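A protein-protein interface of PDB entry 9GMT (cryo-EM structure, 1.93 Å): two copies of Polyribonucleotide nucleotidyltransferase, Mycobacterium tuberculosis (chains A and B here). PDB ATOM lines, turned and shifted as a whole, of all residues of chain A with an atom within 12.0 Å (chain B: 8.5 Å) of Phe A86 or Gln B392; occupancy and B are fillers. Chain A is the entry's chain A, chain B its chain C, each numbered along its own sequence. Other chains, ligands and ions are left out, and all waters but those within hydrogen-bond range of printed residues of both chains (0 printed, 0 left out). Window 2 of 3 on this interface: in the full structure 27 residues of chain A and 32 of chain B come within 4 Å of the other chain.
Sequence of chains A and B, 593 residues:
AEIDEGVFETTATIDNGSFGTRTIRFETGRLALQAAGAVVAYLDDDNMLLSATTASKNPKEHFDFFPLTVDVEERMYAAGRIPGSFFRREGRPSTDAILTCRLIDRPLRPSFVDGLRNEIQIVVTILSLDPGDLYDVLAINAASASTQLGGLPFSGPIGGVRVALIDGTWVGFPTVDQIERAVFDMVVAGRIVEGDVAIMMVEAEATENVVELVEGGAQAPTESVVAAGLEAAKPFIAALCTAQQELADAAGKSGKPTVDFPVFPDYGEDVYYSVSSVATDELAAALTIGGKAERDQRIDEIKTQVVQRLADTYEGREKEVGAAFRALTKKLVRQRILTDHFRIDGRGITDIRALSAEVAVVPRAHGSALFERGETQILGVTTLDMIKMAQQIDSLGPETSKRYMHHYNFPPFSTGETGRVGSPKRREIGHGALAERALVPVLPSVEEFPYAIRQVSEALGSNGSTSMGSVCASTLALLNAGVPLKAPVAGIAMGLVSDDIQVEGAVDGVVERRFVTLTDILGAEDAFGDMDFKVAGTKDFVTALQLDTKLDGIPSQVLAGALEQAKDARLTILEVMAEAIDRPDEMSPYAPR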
ATOM      1  N   MET A  76     -35.545  12.570   5.079  1.00  0.00           N
ATOM      2  CA  MET A  76     -36.439  13.703   5.278  1.00  0.00           C
ATOM      3  C   MET A  76     -37.165  14.114   4.005  1.00  0.00           C
ATOM      4  O   MET A  76     -38.272  14.652   4.092  1.00  0.00           O
ATOM      5  CB  MET A  76     -35.672  14.896   5.836  1.00  0.00           C
ATOM      6  CG  MET A  76     -35.711  14.996   7.334  1.00  0.00           C
ATOM      7  SD  MET A  76     -37.384  15.147   7.972  1.00  0.00           S
ATOM      8  CE  MET A  76     -37.119  14.591   9.641  1.00  0.00           C
ATOM      9  N   ILE A  82     -36.557  19.870   4.615  1.00  0.00           N
ATOM     10  CA  ILE A  82     -35.109  19.872   4.819  1.00  0.00           C
ATOM     11  C   ILE A  82     -34.826  19.638   6.299  1.00  0.00           C
ATOM     12  O   ILE A  82     -35.515  20.212   7.152  1.00  0.00           O
ATOM     13  CB  ILE A  82     -34.471  21.182   4.327  1.00  0.00           C
ATOM     14  CG1 ILE A  82     -34.596  21.301   2.810  1.00  0.00           C
ATOM     15  CG2 ILE A  82     -33.013  21.278   4.758  1.00  0.00           C
ATOM     16  CD1 ILE A  82     -33.941  22.525   2.242  1.00  0.00           C
ATOM     17  N   PRO A  83     -33.836  18.816   6.648  1.00  0.00           N
ATOM     18  CA  PRO A  83     -33.564  18.540   8.066  1.00  0.00           C
ATOM     19  C   PRO A  83     -33.206  19.802   8.838  1.00  0.00           C
ATOM     20  O   PRO A  83     -32.551  20.707   8.321  1.00  0.00           O
ATOM     21  CB  PRO A  83     -32.388  17.561   8.020  1.00  0.00           C
ATOM     22  CG  PRO A  83     -32.410  16.988   6.659  1.00  0.00           C
ATOM     23  CD  PRO A  83     -32.976  18.028   5.754  1.00  0.00           C
ATOM     24  N   GLY A  84     -33.655  19.858  10.087  1.00  0.00           N
ATOM     25  CA  GLY A  84     -33.476  21.019  10.928  1.00  0.00           C
ATOM     26  C   GLY A  84     -32.192  21.094  11.719  1.00  0.00           C
ATOM     27  O   GLY A  84     -31.976  22.083  12.418  1.00  0.00           O
ATOM     28  N   SER A  85     -31.325  20.090  11.640  1.00  0.00           N
ATOM     29  CA  SER A  85     -30.087  20.115  12.401  1.00  0.00           C
ATOM     30  C   SER A  85     -29.119  21.143  11.816  1.00  0.00           C
ATOM     31  O   SER A  85     -29.334  21.702  10.740  1.00  0.00           O
ATOM     32  CB  SER A  85     -29.450  18.729  12.434  1.00  0.00           C
ATOM     33  OG  SER A  85     -29.204  18.249  11.129  1.00  0.00           O
ATOM     34  N   PHE A  86     -28.036  21.395  12.554  1.00  0.00           N
ATOM     35  CA  PHE A  86     -27.107  22.454  12.172  1.00  0.00           C
ATOM     36  C   PHE A  86     -26.433  22.168  10.837  1.00  0.00           C
ATOM     37  O   PHE A  86     -26.227  23.089  10.041  1.00  0.00           O
ATOM     38  CB  PHE A  86     -26.059  22.658  13.268  1.00  0.00           C
ATOM     39  CG  PHE A  86     -25.153  23.836  13.035  1.00  0.00           C
ATOM     40  CD1 PHE A  86     -25.644  25.125  13.085  1.00  0.00           C
ATOM     41  CD2 PHE A  86     -23.811  23.652  12.769  1.00  0.00           C
ATOM     42  CE1 PHE A  86     -24.816  26.204  12.872  1.00  0.00           C
ATOM     43  CE2 PHE A  86     -22.981  24.730  12.555  1.00  0.00           C
ATOM     44  CZ  PHE A  86     -23.483  26.005  12.607  1.00  0.00           C
ATOM     45  N   PHE A  87     -26.089  20.913  10.567  1.00  0.00           N
ATOM     46  CA  PHE A  87     -25.446  20.553   9.312  1.00  0.00           C
ATOM     47  C   PHE A  87     -26.427  20.106   8.232  1.00  0.00           C
ATOM     48  O   PHE A  87     -25.990  19.755   7.134  1.00  0.00           O
ATOM     49  CB  PHE A  87     -24.390  19.472   9.556  1.00  0.00           C
ATOM     50  CG  PHE A  87     -23.254  19.933  10.422  1.00  0.00           C
ATOM     51  CD1 PHE A  87     -22.290  20.788   9.919  1.00  0.00           C
ATOM     52  CD2 PHE A  87     -23.154  19.527  11.737  1.00  0.00           C
ATOM     53  CE1 PHE A  87     -21.249  21.227  10.708  1.00  0.00           C
ATOM     54  CE2 PHE A  87     -22.114  19.961  12.532  1.00  0.00           C
ATOM     55  CZ  PHE A  87     -21.160  20.811  12.015  1.00  0.00           C
ATOM     56  N   ARG A  88     -27.730  20.116   8.512  1.00  0.00           N
ATOM     57  CA  ARG A  88     -28.767  19.928   7.493  1.00  0.00           C
ATOM     58  C   ARG A  88     -28.721  18.537   6.866  1.00  0.00           C
ATOM     59  O   ARG A  88     -29.088  18.354   5.706  1.00  0.00           O
ATOM     60  CB  ARG A  88     -28.672  21.003   6.409  1.00  0.00           C
ATOM     61  CG  ARG A  88     -28.799  22.426   6.910  1.00  0.00           C
ATOM     62  CD  ARG A  88     -30.224  22.738   7.303  1.00  0.00           C
ATOM     63  NE  ARG A  88     -30.453  24.167   7.470  1.00  0.00           N
ATOM     64  CZ  ARG A  88     -30.573  24.777   8.639  1.00  0.00           C
ATOM     65  NH1 ARG A  88     -30.518  24.107   9.777  1.00  0.00           N
ATOM     66  NH2 ARG A  88     -30.754  26.092   8.668  1.00  0.00           N
ATOM     67  N   ARG A  89     -28.287  17.545   7.635  1.00  0.00           N
ATOM     68  CA  ARG A  89     -28.171  16.187   7.129  1.00  0.00           C
ATOM     69  C   ARG A  89     -28.621  15.222   8.215  1.00  0.00           C
ATOM     70  O   ARG A  89     -28.497  15.509   9.406  1.00  0.00           O
ATOM     71  CB  ARG A  89     -26.734  15.885   6.675  1.00  0.00           C
ATOM     72  CG  ARG A  89     -26.576  14.637   5.829  1.00  0.00           C
ATOM     73  CD  ARG A  89     -25.216  14.587   5.144  1.00  0.00           C
ATOM     74  NE  ARG A  89     -25.075  13.408   4.299  1.00  0.00           N
ATOM     75  CZ  ARG A  89     -24.147  13.252   3.366  1.00  0.00           C
ATOM     76  NH1 ARG A  89     -23.250  14.189   3.119  1.00  0.00           N
ATOM     77  NH2 ARG A  89     -24.125  12.129   2.657  1.00  0.00           N
ATOM     78  N   GLU A  90     -29.157  14.081   7.793  1.00  0.00           N
ATOM     79  CA  GLU A  90     -29.601  13.070   8.744  1.00  0.00           C
ATOM     80  C   GLU A  90     -28.409  12.473   9.479  1.00  0.00           C
ATOM     81  O   GLU A  90     -27.377  12.175   8.875  1.00  0.00           O
ATOM     82  CB  GLU A  90     -30.381  11.970   8.023  1.00  0.00           C
ATOM     83  CG  GLU A  90     -31.663  12.438   7.357  1.00  0.00           C
ATOM     84  CD  GLU A  90     -31.459  12.831   5.906  1.00  0.00           C
ATOM     85  OE1 GLU A  90     -30.299  12.847   5.454  1.00  0.00           O
ATOM     86  OE2 GLU A  90     -32.455  13.126   5.222  1.00  0.00           O
ATOM     87  N   GLY A  91     -28.556  12.287  10.787  1.00  0.00           N
ATOM     88  CA  GLY A  91     -27.473  11.766  11.597  1.00  0.00           C
ATOM     89  C   GLY A  91     -27.746  10.408  12.209  1.00  0.00           C
ATOM     90  O   GLY A  91     -28.037   9.446  11.496  1.00  0.00           O
ATOM     91  N   ARG A  92     -27.638  10.318  13.531  1.00  0.00           N
ATOM     92  CA  ARG A  92     -27.883   9.061  14.216  1.00  0.00           C
ATOM     93  C   ARG A  92     -29.373   8.720  14.183  1.00  0.00           C
ATOM     94  O   ARG A  92     -30.222   9.613  14.169  1.00  0.00           O
ATOM     95  CB  ARG A  92     -27.395   9.135  15.659  1.00  0.00           C
ATOM     96  CG  ARG A  92     -25.906   9.399  15.794  1.00  0.00           C
ATOM     97  CD  ARG A  92     -25.087   8.116  15.758  1.00  0.00           C
ATOM     98  NE  ARG A  92     -25.190   7.436  14.473  1.00  0.00           N
ATOM     99  CZ  ARG A  92     -24.383   7.647  13.442  1.00  0.00           C
ATOM    100  NH1 ARG A  92     -23.391   8.519  13.509  1.00  0.00           N
ATOM    101  NH2 ARG A  92     -24.579   6.968  12.315  1.00  0.00           N
ATOM    102  N   ASP A 394     -38.413  16.213  15.849  1.00  0.00           N
ATOM    103  CA  ASP A 394     -38.220  16.616  14.459  1.00  0.00           C
ATOM    104  C   ASP A 394     -37.995  15.387  13.587  1.00  0.00           C
ATOM    105  O   ASP A 394     -36.982  15.249  12.902  1.00  0.00           O
ATOM    106  CB  ASP A 394     -37.066  17.606  14.334  1.00  0.00           C
ATOM    107  CG  ASP A 394     -36.917  18.157  12.926  1.00  0.00           C
ATOM    108  OD1 ASP A 394     -37.911  18.668  12.373  1.00  0.00           O
ATOM    109  OD2 ASP A 394     -35.803  18.079  12.371  1.00  0.00           O
ATOM    110  N   GLY B  84     -18.209  29.232  17.998  1.00  0.00           N
ATOM    111  CA  GLY B  84     -19.605  29.441  18.314  1.00  0.00           C
ATOM    112  C   GLY B  84     -20.359  28.256  18.868  1.00  0.00           C
ATOM    113  O   GLY B  84     -21.532  28.401  19.216  1.00  0.00           O
ATOM    114  N   SER B  85     -19.733  27.090  18.977  1.00  0.00           N
ATOM    115  CA  SER B  85     -20.438  25.919  19.469  1.00  0.00           C
ATOM    116  C   SER B  85     -20.718  26.048  20.966  1.00  0.00           C
ATOM    117  O   SER B  85     -20.271  26.979  21.638  1.00  0.00           O
ATOM    118  CB  SER B  85     -19.642  24.650  19.178  1.00  0.00           C
ATOM    119  OG  SER B  85     -18.303  24.771  19.607  1.00  0.00           O
ATOM    120  N   ILE B 387     -36.126  30.207   2.267  1.00  0.00           N
ATOM    121  CA  ILE B 387     -34.728  30.623   2.193  1.00  0.00           C
ATOM    122  C   ILE B 387     -34.053  30.596   3.557  1.00  0.00           C
ATOM    123  O   ILE B 387     -32.825  30.494   3.644  1.00  0.00           O
ATOM    124  CB  ILE B 387     -34.620  32.014   1.541  1.00  0.00           C
ATOM    125  CG1 ILE B 387     -33.225  32.213   0.956  1.00  0.00           C
ATOM    126  CG2 ILE B 387     -34.931  33.096   2.545  1.00  0.00           C
ATOM    127  CD1 ILE B 387     -32.957  31.379  -0.260  1.00  0.00           C
ATOM    128  N   LYS B 388     -34.824  30.675   4.639  1.00  0.00           N
ATOM    129  CA  LYS B 388     -34.235  30.592   5.969  1.00  0.00           C
ATOM    130  C   LYS B 388     -33.676  29.211   6.287  1.00  0.00           C
ATOM    131  O   LYS B 388     -32.960  29.070   7.281  1.00  0.00           O
ATOM    132  CB  LYS B 388     -35.266  30.985   7.025  1.00  0.00           C
ATOM    133  CG  LYS B 388     -36.198  29.860   7.415  1.00  0.00           C
ATOM    134  CD  LYS B 388     -37.200  30.307   8.452  1.00  0.00           C
ATOM    135  CE  LYS B 388     -38.319  29.297   8.596  1.00  0.00           C
ATOM    136  NZ  LYS B 388     -38.075  28.358   9.720  1.00  0.00           N
ATOM    137  N   MET B 389     -33.979  28.197   5.483  1.00  0.00           N
ATOM    138  CA  MET B 389     -33.456  26.858   5.701  1.00  0.00           C
ATOM    139  C   MET B 389     -32.106  26.634   5.031  1.00  0.00           C
ATOM    140  O   MET B 389     -31.600  25.510   5.055  1.00  0.00           O
ATOM    141  CB  MET B 389     -34.461  25.811   5.214  1.00  0.00           C
ATOM    142  CG  MET B 389     -35.749  25.750   6.027  1.00  0.00           C
ATOM    143  SD  MET B 389     -35.500  25.655   7.811  1.00  0.00           S
ATOM    144  CE  MET B 389     -34.529  24.165   7.951  1.00  0.00           C
ATOM    145  N   ALA B 390     -31.519  27.664   4.430  1.00  0.00           N
ATOM    146  CA  ALA B 390     -30.157  27.558   3.926  1.00  0.00           C
ATOM    147  C   ALA B 390     -29.194  27.280   5.073  1.00  0.00           C
ATOM    148  O   ALA B 390     -29.392  27.728   6.202  1.00  0.00           O
ATOM    149  CB  ALA B 390     -29.751  28.840   3.204  1.00  0.00           C
ATOM    150  N   GLN B 391     -28.140  26.528   4.776  1.00  0.00           N
ATOM    151  CA  GLN B 391     -27.181  26.157   5.806  1.00  0.00           C
ATOM    152  C   GLN B 391     -26.366  27.367   6.251  1.00  0.00           C
ATOM    153  O   GLN B 391     -25.839  28.115   5.424  1.00  0.00           O
ATOM    154  CB  GLN B 391     -26.258  25.053   5.299  1.00  0.00           C
ATOM    155  CG  GLN B 391     -25.241  24.599   6.323  1.00  0.00           C
ATOM    156  CD  GLN B 391     -24.382  23.460   5.838  1.00  0.00           C
ATOM    157  OE1 GLN B 391     -24.550  22.974   4.725  1.00  0.00           O
ATOM    158  NE2 GLN B 391     -23.449  23.027   6.670  1.00  0.00           N
ATOM    159  N   GLN B 392     -26.267  27.553   7.564  1.00  0.00           N
ATOM    160  CA  GLN B 392     -25.429  28.587   8.156  1.00  0.00           C
ATOM    161  C   GLN B 392     -24.080  27.972   8.498  1.00  0.00           C
ATOM    162  O   GLN B 392     -24.019  26.950   9.188  1.00  0.00           O
ATOM    163  CB  GLN B 392     -26.087  29.168   9.407  1.00  0.00           C
ATOM    164  CG  GLN B 392     -27.502  29.692   9.198  1.00  0.00           C
ATOM    165  CD  GLN B 392     -27.596  30.733   8.100  1.00  0.00           C
ATOM    166  OE1 GLN B 392     -26.847  31.707   8.087  1.00  0.00           O
ATOM    167  NE2 GLN B 392     -28.522  30.530   7.172  1.00  0.00           N
ATOM    168  N   ILE B 393     -23.002  28.585   8.024  1.00  0.00           N
ATOM    169  CA  ILE B 393     -21.660  28.030   8.154  1.00  0.00           C
ATOM    170  C   ILE B 393     -20.832  28.922   9.068  1.00  0.00           C
ATOM    171  O   ILE B 393     -20.864  30.151   8.945  1.00  0.00           O
ATOM    172  CB  ILE B 393     -20.989  27.867   6.781  1.00  0.00           C
ATOM    173  CG1 ILE B 393     -21.633  26.709   6.022  1.00  0.00           C
ATOM    174  CG2 ILE B 393     -19.509  27.618   6.945  1.00  0.00           C
ATOM    175  CD1 ILE B 393     -21.711  26.924   4.548  1.00  0.00           C
ATOM    176  N   ASP B 394     -20.091  28.301   9.981  1.00  0.00           N
ATOM    177  CA  ASP B 394     -19.220  28.985  10.937  1.00  0.00           C
ATOM    178  C   ASP B 394     -17.841  28.333  10.852  1.00  0.00           C
ATOM    179  O   ASP B 394     -17.562  27.365  11.561  1.00  0.00           O
ATOM    180  CB  ASP B 394     -19.804  28.904  12.347  1.00  0.00           C
ATOM    181  CG  ASP B 394     -18.998  29.687  13.365  1.00  0.00           C
ATOM    182  OD1 ASP B 394     -18.621  30.839  13.073  1.00  0.00           O
ATOM    183  OD2 ASP B 394     -18.746  29.153  14.462  1.00  0.00           O
ATOM    184  N   SER B 395     -16.979  28.862   9.987  1.00  0.00           N
ATOM    185  CA  SER B 395     -15.699  28.235   9.690  1.00  0.00           C
ATOM    186  C   SER B 395     -14.643  29.308   9.453  1.00  0.00           C
ATOM    187  O   SER B 395     -14.934  30.506   9.448  1.00  0.00           O
ATOM    188  CB  SER B 395     -15.820  27.306   8.479  1.00  0.00           C
ATOM    189  OG  SER B 395     -16.036  28.059   7.298  1.00  0.00           O
ATOM    190  N   GLU B 399     -16.627  31.780   3.349  1.00  0.00           N
ATOM    191  CA  GLU B 399     -18.014  31.410   3.093  1.00  0.00           C
ATOM    192  C   GLU B 399     -18.838  31.456   4.376  1.00  0.00           C
ATOM    193  O   GLU B 399     -18.367  31.066   5.447  1.00  0.00           O
ATOM    194  CB  GLU B 399     -18.073  30.012   2.476  1.00  0.00           C
ATOM    195  CG  GLU B 399     -19.405  29.310   2.629  1.00  0.00           C
ATOM    196  CD  GLU B 399     -19.475  28.016   1.839  1.00  0.00           C
ATOM    197  OE1 GLU B 399     -18.769  27.055   2.205  1.00  0.00           O
ATOM    198  OE2 GLU B 399     -20.237  27.960   0.852  1.00  0.00           O
ATOM    199  N   THR B 400     -20.081  31.930   4.263  1.00  0.00           N
ATOM    200  CA  THR B 400     -20.954  32.071   5.422  1.00  0.00           C
ATOM    201  C   THR B 400     -22.280  31.324   5.326  1.00  0.00           C
ATOM    202  O   THR B 400     -22.894  31.082   6.369  1.00  0.00           O
ATOM    203  CB  THR B 400     -21.256  33.553   5.696  1.00  0.00           C
ATOM    204  OG1 THR B 400     -21.671  34.195   4.487  1.00  0.00           O
ATOM    205  CG2 THR B 400     -20.030  34.255   6.247  1.00  0.00           C
ATOM    206  N   SER B 401     -22.747  30.966   4.132  1.00  0.00           N
ATOM    207  CA  SER B 401     -24.001  30.232   4.011  1.00  0.00           C
ATOM    208  C   SER B 401     -24.055  29.522   2.666  1.00  0.00           C
ATOM    209  O   SER B 401     -23.368  29.897   1.717  1.00  0.00           O
ATOM    210  CB  SER B 401     -25.206  31.161   4.185  1.00  0.00           C
ATOM    211  OG  SER B 401     -25.580  31.752   2.960  1.00  0.00           O
ATOM    212  N   LYS B 402     -24.893  28.486   2.594  1.00  0.00           N
ATOM    213  CA  LYS B 402     -25.062  27.682   1.385  1.00  0.00           C
ATOM    214  C   LYS B 402     -26.539  27.608   1.028  1.00  0.00           C
ATOM    215  O   LYS B 402     -27.332  27.019   1.766  1.00  0.00           O
ATOM    216  CB  LYS B 402     -24.495  26.275   1.565  1.00  0.00           C
ATOM    217  CG  LYS B 402     -22.995  26.202   1.614  1.00  0.00           C
ATOM    218  CD  LYS B 402     -22.524  24.785   1.897  1.00  0.00           C
ATOM    219  CE  LYS B 402     -22.725  23.872   0.712  1.00  0.00           C
ATOM    220  NZ  LYS B 402     -21.810  24.234  -0.394  1.00  0.00           N
ATOM    221  N   ARG B 403     -26.900  28.190  -0.112  1.00  0.00           N
ATOM    222  CA  ARG B 403     -28.254  28.090  -0.640  1.00  0.00           C
ATOM    223  C   ARG B 403     -28.536  26.755  -1.318  1.00  0.00           C
ATOM    224  O   ARG B 403     -29.675  26.282  -1.282  1.00  0.00           O
ATOM    225  CB  ARG B 403     -28.501  29.244  -1.607  1.00  0.00           C
ATOM    226  CG  ARG B 403     -29.796  29.184  -2.366  1.00  0.00           C
ATOM    227  CD  ARG B 403     -29.935  30.436  -3.182  1.00  0.00           C
ATOM    228  NE  ARG B 403     -31.076  30.424  -4.088  1.00  0.00           N
ATOM    229  CZ  ARG B 403     -31.004  30.076  -5.365  1.00  0.00           C
ATOM    230  NH1 ARG B 403     -29.854  29.746  -5.925  1.00  0.00           N
ATOM    231  NH2 ARG B 403     -32.107  30.089  -6.104  1.00  0.00           N
ATOM    232  N   MET B 405     -27.410  22.722  -1.586  1.00  0.00           N
ATOM    233  CA  MET B 405     -26.674  21.648  -0.929  1.00  0.00           C
ATOM    234  C   MET B 405     -26.842  20.343  -1.694  1.00  0.00           C
ATOM    235  O   MET B 405     -27.911  20.072  -2.241  1.00  0.00           O
ATOM    236  CB  MET B 405     -27.131  21.469   0.526  1.00  0.00           C
ATOM    237  CG  MET B 405     -27.150  22.752   1.336  1.00  0.00           C
ATOM    238  SD  MET B 405     -28.250  22.719   2.762  1.00  0.00           S
ATOM    239  CE  MET B 405     -29.675  23.585   2.131  1.00  0.00           C
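The backbone carbonyl oxygen of Met B389 lies within hydrogen-bond range of the guanidinium group of Arg A88, at 3.0 Å. NH2 of Arg A88 lies within hydrogen-bond range of O of Ala B390 (3.3 Å).
O of Gln B391 is in hydrogen-bond range of N of Lys B402, 3.0 Å away. NH1 of Arg A88 sits at hydrogen-bond distance from O of Ser A85, 2.8 Å away. The backbone carbonyl oxygen (O) of Ala B390 is in hydrogen-bond range of the side-chain amide nitrogen (NE2) of Gln B392, 3.1 Å away.
Among the printed residues, merely in contact across the chains: Phe A86 with Gln B392, Arg A88 with Lys B388 and Arg A88 with Gln B391.
No residue of chain B comes within 4 Å of Ser A85. No residue of chain B comes within 4 Å of Phe A87. No residue of chain A comes within 4 Å of Ile B393. No residue of chain A comes within 4 Å of Asp B394. Thr B400 touches none of the printed residues of chain A. No residue of chain A comes within 4 Å of Ser B401. Printed residues of chain A within 4 Å of Gln B391: Arg A88 (3.99 Å). Of the printed residues of chain B, Arg A88 touches Lys B388, Met B389, Ala B390 and Gln B391. Printed residues of chain A within 4 Å of Lys B388: Arg A88 (3.96 Å).
Printed residues of chain B that touch a printed residue of chain A: Lys B388, Met B389, Ala B390, Gln B391 and Gln B392. Along chain B the printed residues that touch a printed residue of chain A span positions 388 to 392. Printed residues of chain A that touch a printed residue of chain B: Phe A86 and Arg A88. Hydrophobic or aromatic side chains of chain A that line the printed part of chain B: Phe A86. Among the printed residues, 5 pairs touch across the chains. Among the printed residues, no Asp or Glu carboxylate lies within 4 Å of a Lys or Arg side-chain nitrogen of the other chain.
Positions printed for both chains: 84, 85 and 394. Of the 5 pairs that touch across the chains among the printed residues, none has its exchanged pair printed and touching as well.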
